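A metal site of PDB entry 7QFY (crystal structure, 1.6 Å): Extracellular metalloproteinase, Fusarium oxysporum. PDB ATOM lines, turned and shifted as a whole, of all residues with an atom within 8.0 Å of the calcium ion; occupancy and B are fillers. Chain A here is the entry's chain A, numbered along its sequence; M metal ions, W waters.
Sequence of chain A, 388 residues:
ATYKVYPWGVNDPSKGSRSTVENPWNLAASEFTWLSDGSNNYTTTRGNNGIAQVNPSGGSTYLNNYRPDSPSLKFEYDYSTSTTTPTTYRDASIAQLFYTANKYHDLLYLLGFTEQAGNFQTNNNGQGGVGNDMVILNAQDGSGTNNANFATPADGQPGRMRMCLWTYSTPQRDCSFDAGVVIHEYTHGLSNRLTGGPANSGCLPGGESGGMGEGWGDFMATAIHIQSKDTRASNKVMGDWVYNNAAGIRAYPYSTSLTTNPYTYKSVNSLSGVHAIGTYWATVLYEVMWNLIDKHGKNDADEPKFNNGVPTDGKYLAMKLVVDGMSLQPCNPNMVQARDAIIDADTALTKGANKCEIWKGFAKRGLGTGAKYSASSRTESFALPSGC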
ATOM      1  N   ALA A 117      21.763   8.663 -15.806  1.00  0.00           N
ATOM      2  CA  ALA A 117      23.129   9.156 -15.610  1.00  0.00           C
ATOM      3  C   ALA A 117      23.154  10.534 -14.959  1.00  0.00           C
ATOM      4  O   ALA A 117      24.252  11.092 -14.748  1.00  0.00           O
ATOM      5  CB  ALA A 117      23.868   9.215 -16.968  1.00  0.00           C
ATOM      6  N   GLY A 118      21.991  11.085 -14.618  1.00  0.00           N
ATOM      7  CA  GLY A 118      21.940  12.360 -13.928  1.00  0.00           C
ATOM      8  C   GLY A 118      21.899  13.572 -14.834  1.00  0.00           C
ATOM      9  O   GLY A 118      22.448  14.614 -14.466  1.00  0.00           O
ATOM     10  N   THR A 152      26.045  23.819 -11.071  1.00  0.00           N
ATOM     11  CA  THR A 152      25.516  22.460 -11.117  1.00  0.00           C
ATOM     12  C   THR A 152      25.083  21.990  -9.747  1.00  0.00           C
ATOM     13  O   THR A 152      25.916  21.457  -8.991  1.00  0.00           O
ATOM     14  CB  THR A 152      26.539  21.478 -11.682  1.00  0.00           C
ATOM     15  OG1 THR A 152      27.074  21.976 -12.919  1.00  0.00           O
ATOM     16  CG2 THR A 152      25.858  20.168 -11.975  1.00  0.00           C
ATOM     17  N   PRO A 153      23.809  22.092  -9.393  1.00  0.00           N
ATOM     18  CA  PRO A 153      23.351  21.437  -8.171  1.00  0.00           C
ATOM     19  C   PRO A 153      23.190  19.942  -8.410  1.00  0.00           C
ATOM     20  O   PRO A 153      23.348  19.452  -9.527  1.00  0.00           O
ATOM     21  CB  PRO A 153      22.012  22.108  -7.885  1.00  0.00           C
ATOM     22  CG  PRO A 153      21.588  22.739  -9.131  1.00  0.00           C
ATOM     23  CD  PRO A 153      22.710  22.717 -10.124  1.00  0.00           C
ATOM     24  N   ALA A 154      22.906  19.222  -7.331  1.00  0.00           N
ATOM     25  CA  ALA A 154      22.690  17.785  -7.442  1.00  0.00           C
ATOM     26  C   ALA A 154      21.458  17.501  -8.301  1.00  0.00           C
ATOM     27  O   ALA A 154      20.616  18.379  -8.540  1.00  0.00           O
ATOM     28  CB  ALA A 154      22.510  17.141  -6.061  1.00  0.00           C
ATOM     29  N   ASP A 155      21.400  16.248  -8.784  1.00  0.00           N
ATOM     30  CA  ASP A 155      20.302  15.797  -9.618  1.00  0.00           C
ATOM     31  C   ASP A 155      18.965  16.184  -8.993  1.00  0.00           C
ATOM     32  O   ASP A 155      18.737  15.971  -7.800  1.00  0.00           O
ATOM     33  CB  ASP A 155      20.398  14.266  -9.774  1.00  0.00           C
ATOM     34  CG  ASP A 155      19.728  13.742 -11.031  1.00  0.00           C
ATOM     35  OD1 ASP A 155      19.486  14.549 -11.929  1.00  0.00           O
ATOM     36  OD2 ASP A 155      19.446  12.516 -11.111  1.00  0.00           O
ATOM     37  N   GLY A 189      28.292  21.061 -16.272  1.00  0.00           N
ATOM     38  CA  GLY A 189      27.175  20.302 -15.728  1.00  0.00           C
ATOM     39  C   GLY A 189      27.361  18.819 -15.937  1.00  0.00           C
ATOM     40  O   GLY A 189      27.099  18.022 -15.035  1.00  0.00           O
ATOM     41  N   LEU A 190      27.852  18.428 -17.110  1.00  0.00           N
ATOM     42  CA  LEU A 190      28.148  17.028 -17.386  1.00  0.00           C
ATOM     43  C   LEU A 190      29.156  16.460 -16.400  1.00  0.00           C
ATOM     44  O   LEU A 190      28.920  15.404 -15.788  1.00  0.00           O
ATOM     45  CB  LEU A 190      28.674  16.896 -18.816  1.00  0.00           C
ATOM     46  CG  LEU A 190      29.191  15.532 -19.248  1.00  0.00           C
ATOM     47  CD1 LEU A 190      28.059  14.517 -19.451  1.00  0.00           C
ATOM     48  CD2 LEU A 190      30.068  15.631 -20.507  1.00  0.00           C
ATOM     49  N   SER A 191      30.286  17.129 -16.225  1.00  0.00           N
ATOM     50  CA  SER A 191      31.353  16.543 -15.414  1.00  0.00           C
ATOM     51  C   SER A 191      31.005  16.576 -13.941  1.00  0.00           C
ATOM     52  O   SER A 191      31.355  15.665 -13.196  1.00  0.00           O
ATOM     53  CB  SER A 191      32.674  17.275 -15.672  1.00  0.00           C
ATOM     54  OG  SER A 191      32.543  18.631 -15.339  1.00  0.00           O
ATOM     55  N   ASN A 192      30.308  17.622 -13.495  1.00  0.00           N
ATOM     56  CA  ASN A 192      29.922  17.661 -12.093  1.00  0.00           C
ATOM     57  C   ASN A 192      28.856  16.616 -11.778  1.00  0.00           C
ATOM     58  O   ASN A 192      28.897  16.000 -10.705  1.00  0.00           O
ATOM     59  CB  ASN A 192      29.451  19.051 -11.696  1.00  0.00           C
ATOM     60  CG  ASN A 192      30.578  19.939 -11.243  1.00  0.00           C
ATOM     61  OD1 ASN A 192      31.312  19.614 -10.306  1.00  0.00           O
ATOM     62  ND2 ASN A 192      30.725  21.087 -11.886  1.00  0.00           N
ATOM     63  N   ARG A 193      27.911  16.371 -12.690  1.00  0.00           N
ATOM     64  CA  ARG A 193      26.910  15.336 -12.445  1.00  0.00           C
ATOM     65  C   ARG A 193      27.543  13.949 -12.457  1.00  0.00           C
ATOM     66  O   ARG A 193      27.342  13.155 -11.547  1.00  0.00           O
ATOM     67  CB  ARG A 193      25.766  15.424 -13.450  1.00  0.00           C
ATOM     68  CG  ARG A 193      24.809  16.606 -13.212  1.00  0.00           C
ATOM     69  CD  ARG A 193      23.924  16.370 -11.987  1.00  0.00           C
ATOM     70  NE  ARG A 193      23.096  17.523 -11.646  1.00  0.00           N
ATOM     71  CZ  ARG A 193      21.887  17.746 -12.134  1.00  0.00           C
ATOM     72  NH1 ARG A 193      21.359  16.980 -13.077  1.00  0.00           N
ATOM     73  NH2 ARG A 193      21.181  18.756 -11.654  1.00  0.00           N
ATOM     74  N   LEU A 194      28.329  13.641 -13.503  1.00  0.00           N
ATOM     75  CA  LEU A 194      28.883  12.299 -13.623  1.00  0.00           C
ATOM     76  C   LEU A 194      29.888  11.996 -12.517  1.00  0.00           C
ATOM     77  O   LEU A 194      29.905  10.878 -11.988  1.00  0.00           O
ATOM     78  CB  LEU A 194      29.510  12.102 -14.993  1.00  0.00           C
ATOM     79  CG  LEU A 194      28.519  12.064 -16.160  1.00  0.00           C
ATOM     80  CD1 LEU A 194      29.253  11.707 -17.424  1.00  0.00           C
ATOM     81  CD2 LEU A 194      27.381  11.046 -15.886  1.00  0.00           C
ATOM     82  N   THR A 195      30.762  12.944 -12.175  1.00  0.00           N
ATOM     83  CA  THR A 195      31.807  12.640 -11.208  1.00  0.00           C
ATOM     84  C   THR A 195      31.199  12.437  -9.823  1.00  0.00           C
ATOM     85  O   THR A 195      30.481  13.304  -9.325  1.00  0.00           O
ATOM     86  CB  THR A 195      32.846  13.760 -11.186  1.00  0.00           C
ATOM     87  OG1 THR A 195      33.358  13.947 -12.519  1.00  0.00           O
ATOM     88  CG2 THR A 195      33.977  13.423 -10.241  1.00  0.00           C
ATOM     89  N   GLY A 196      31.457  11.287  -9.217  1.00  0.00           N
ATOM     90  CA  GLY A 196      30.842  10.995  -7.917  1.00  0.00           C
ATOM     91  C   GLY A 196      29.359  10.710  -8.008  1.00  0.00           C
ATOM     92  O   GLY A 196      28.685  10.633  -6.961  1.00  0.00           O
ATOM     93  N   GLY A 197      28.838  10.548  -9.216  1.00  0.00           N
ATOM     94  CA  GLY A 197      27.445  10.230  -9.428  1.00  0.00           C
ATOM     95  C   GLY A 197      26.571  11.449  -9.234  1.00  0.00           C
ATOM     96  O   GLY A 197      27.013  12.474  -8.711  1.00  0.00           O
ATOM     97  N   PRO A 198      25.285  11.349  -9.606  1.00  0.00           N
ATOM     98  CA  PRO A 198      24.492  12.577  -9.791  1.00  0.00           C
ATOM     99  C   PRO A 198      24.098  13.286  -8.511  1.00  0.00           C
ATOM    100  O   PRO A 198      23.686  14.455  -8.584  1.00  0.00           O
ATOM    101  CB  PRO A 198      23.244  12.081 -10.535  1.00  0.00           C
ATOM    102  CG  PRO A 198      23.673  10.814 -11.206  1.00  0.00           C
ATOM    103  CD  PRO A 198      24.622  10.187 -10.200  1.00  0.00           C
ATOM    104  N   ALA A 199      24.175  12.644  -7.356  1.00  0.00           N
ATOM    105  CA  ALA A 199      23.767  13.288  -6.121  1.00  0.00           C
ATOM    106  C   ALA A 199      24.871  14.131  -5.514  1.00  0.00           C
ATOM    107  O   ALA A 199      24.621  14.875  -4.571  1.00  0.00           O
ATOM    108  CB  ALA A 199      23.285  12.224  -5.115  1.00  0.00           C
ATOM    109  N   ASN A 200      26.084  14.052  -6.059  1.00  0.00           N
ATOM    110  CA  ASN A 200      27.228  14.741  -5.488  1.00  0.00           C
ATOM    111  C   ASN A 200      27.779  15.727  -6.498  1.00  0.00           C
ATOM    112  O   ASN A 200      28.400  15.345  -7.491  1.00  0.00           O
ATOM    113  CB  ASN A 200      28.308  13.756  -5.097  1.00  0.00           C
ATOM    114  CG  ASN A 200      29.081  14.267  -3.952  1.00  0.00           C
ATOM    115  OD1 ASN A 200      29.228  15.486  -3.783  1.00  0.00           O
ATOM    116  ND2 ASN A 200      29.558  13.369  -3.138  1.00  0.00           N
ATOM    117  N   SER A 201      27.557  17.006  -6.229  1.00  0.00           N
ATOM    118  CA  SER A 201      28.060  18.059  -7.093  1.00  0.00           C
ATOM    119  C   SER A 201      29.269  18.755  -6.507  1.00  0.00           C
ATOM    120  O   SER A 201      29.670  19.801  -7.030  1.00  0.00           O
ATOM    121  CB  SER A 201      26.938  19.060  -7.365  1.00  0.00           C
ATOM    122  OG  SER A 201      26.153  18.547  -8.406  1.00  0.00           O
ATOM    123  N   GLY A 202      29.876  18.206  -5.470  1.00  0.00           N
ATOM    124  CA  GLY A 202      31.045  18.838  -4.894  1.00  0.00           C
ATOM    125  C   GLY A 202      32.323  18.112  -5.246  1.00  0.00           C
ATOM    126  O   GLY A 202      33.266  18.124  -4.454  1.00  0.00           O
ATOM    127  N   CYS A 203      32.391  17.490  -6.423  1.00  0.00           N
ATOM    128  CA  CYS A 203      33.514  16.620  -6.704  1.00  0.00           C
ATOM    129  C   CYS A 203      34.620  17.258  -7.519  1.00  0.00           C
ATOM    130  O   CYS A 203      35.662  16.628  -7.704  1.00  0.00           O
ATOM    131  CB  CYS A 203      33.036  15.353  -7.437  1.00  0.00           C
ATOM    132  SG  CYS A 203      32.084  14.223  -6.427  1.00  0.00           S
ATOM    133  N   LEU A 204      34.423  18.482  -8.009  1.00  0.00           N
ATOM    134  CA  LEU A 204      35.419  19.175  -8.839  1.00  0.00           C
ATOM    135  C   LEU A 204      35.586  20.606  -8.376  1.00  0.00           C
ATOM    136  O   LEU A 204      35.451  21.560  -9.155  1.00  0.00           O
ATOM    137  CB  LEU A 204      35.019  19.129 -10.318  1.00  0.00           C
ATOM    138  CG  LEU A 204      34.808  17.759 -10.950  1.00  0.00           C
ATOM    139  CD1 LEU A 204      34.106  17.899 -12.291  1.00  0.00           C
ATOM    140  CD2 LEU A 204      36.110  16.970 -11.087  1.00  0.00           C
ATOM    141  N   MET A 326      34.441   9.878 -16.629  1.00  0.00           N
ATOM    142  CA  MET A 326      33.910  10.692 -15.547  1.00  0.00           C
ATOM    143  C   MET A 326      33.063   9.860 -14.591  1.00  0.00           C
ATOM    144  O   MET A 326      33.039  10.161 -13.390  1.00  0.00           O
ATOM    145  CB  MET A 326      33.063  11.829 -16.097  1.00  0.00           C
ATOM    146  CG  MET A 326      33.795  12.827 -17.001  1.00  0.00           C
ATOM    147  SD  MET A 326      32.622  13.937 -17.802  1.00  0.00           S
ATOM    148  CE  MET A 326      33.726  14.938 -18.826  1.00  0.00           C
ATOM    149  N   CYS A 331      35.493  10.767  -6.695  1.00  0.00           N
ATOM    150  CA  CYS A 331      35.175  12.146  -6.361  1.00  0.00           C
ATOM    151  C   CYS A 331      36.464  12.865  -5.981  1.00  0.00           C
ATOM    152  O   CYS A 331      37.410  12.268  -5.461  1.00  0.00           O
ATOM    153  CB  CYS A 331      34.152  12.176  -5.223  1.00  0.00           C
ATOM    154  SG  CYS A 331      33.342  13.803  -4.891  1.00  0.00           S
HETATM  155 CA    CA M   1      28.267  14.224  -9.473  1.00  0.00          CA
HETATM  156  O   HOH W   1      26.091  15.853  -9.202  1.00  0.00           O
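The side-chain amide oxygen (OD1) of Asn 200 sits at hydrogen-bond distance from the backbone NH (N) of Gly 202 (3.3 Å).
The side-chain hydroxyl of Thr 195 sits at hydrogen-bond distance from the backbone carbonyl oxygen of Ser 191.
The guanidinium group of Arg 193 lies within hydrogen-bond range of the backbone carbonyl oxygen of Ala 154.
The guanidinium group (NE) of Arg 193 sits at hydrogen-bond distance from the backbone carbonyl oxygen (O) of Pro 153 (2.9 Å).
The guanidinium group (NH1) of Arg 193 lies close to the side-chain carboxylate (OD1) of Asp 155 (3.3 Å).
NH1 of Arg 193 is in hydrogen-bond range of O of Gly 118.
The side-chain sulfur (SG) of Cys 203 forms a disulfide with the side-chain sulfur (SG) of Cys 331 (2.0 Å).
Merely in contact with the calcium ion: Gly 196 (3.96 Å).
Of the 24 residues printed, 6 come within 4 Å of the calcium ion.
The nearest printed residue that does not touch the calcium ion is Leu 194 (4.1 Å).
The calcium ion is bound by O of Asn 192, O of Asn 200, O of Gly 197, O of Thr 195, O of Arg 193 and water W1.
The calcium ion has six donor atoms within binding distance.
Water W1 bridges OG of Ser 201 (2.8 Å) and O of Pro 198 (2.8 Å).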
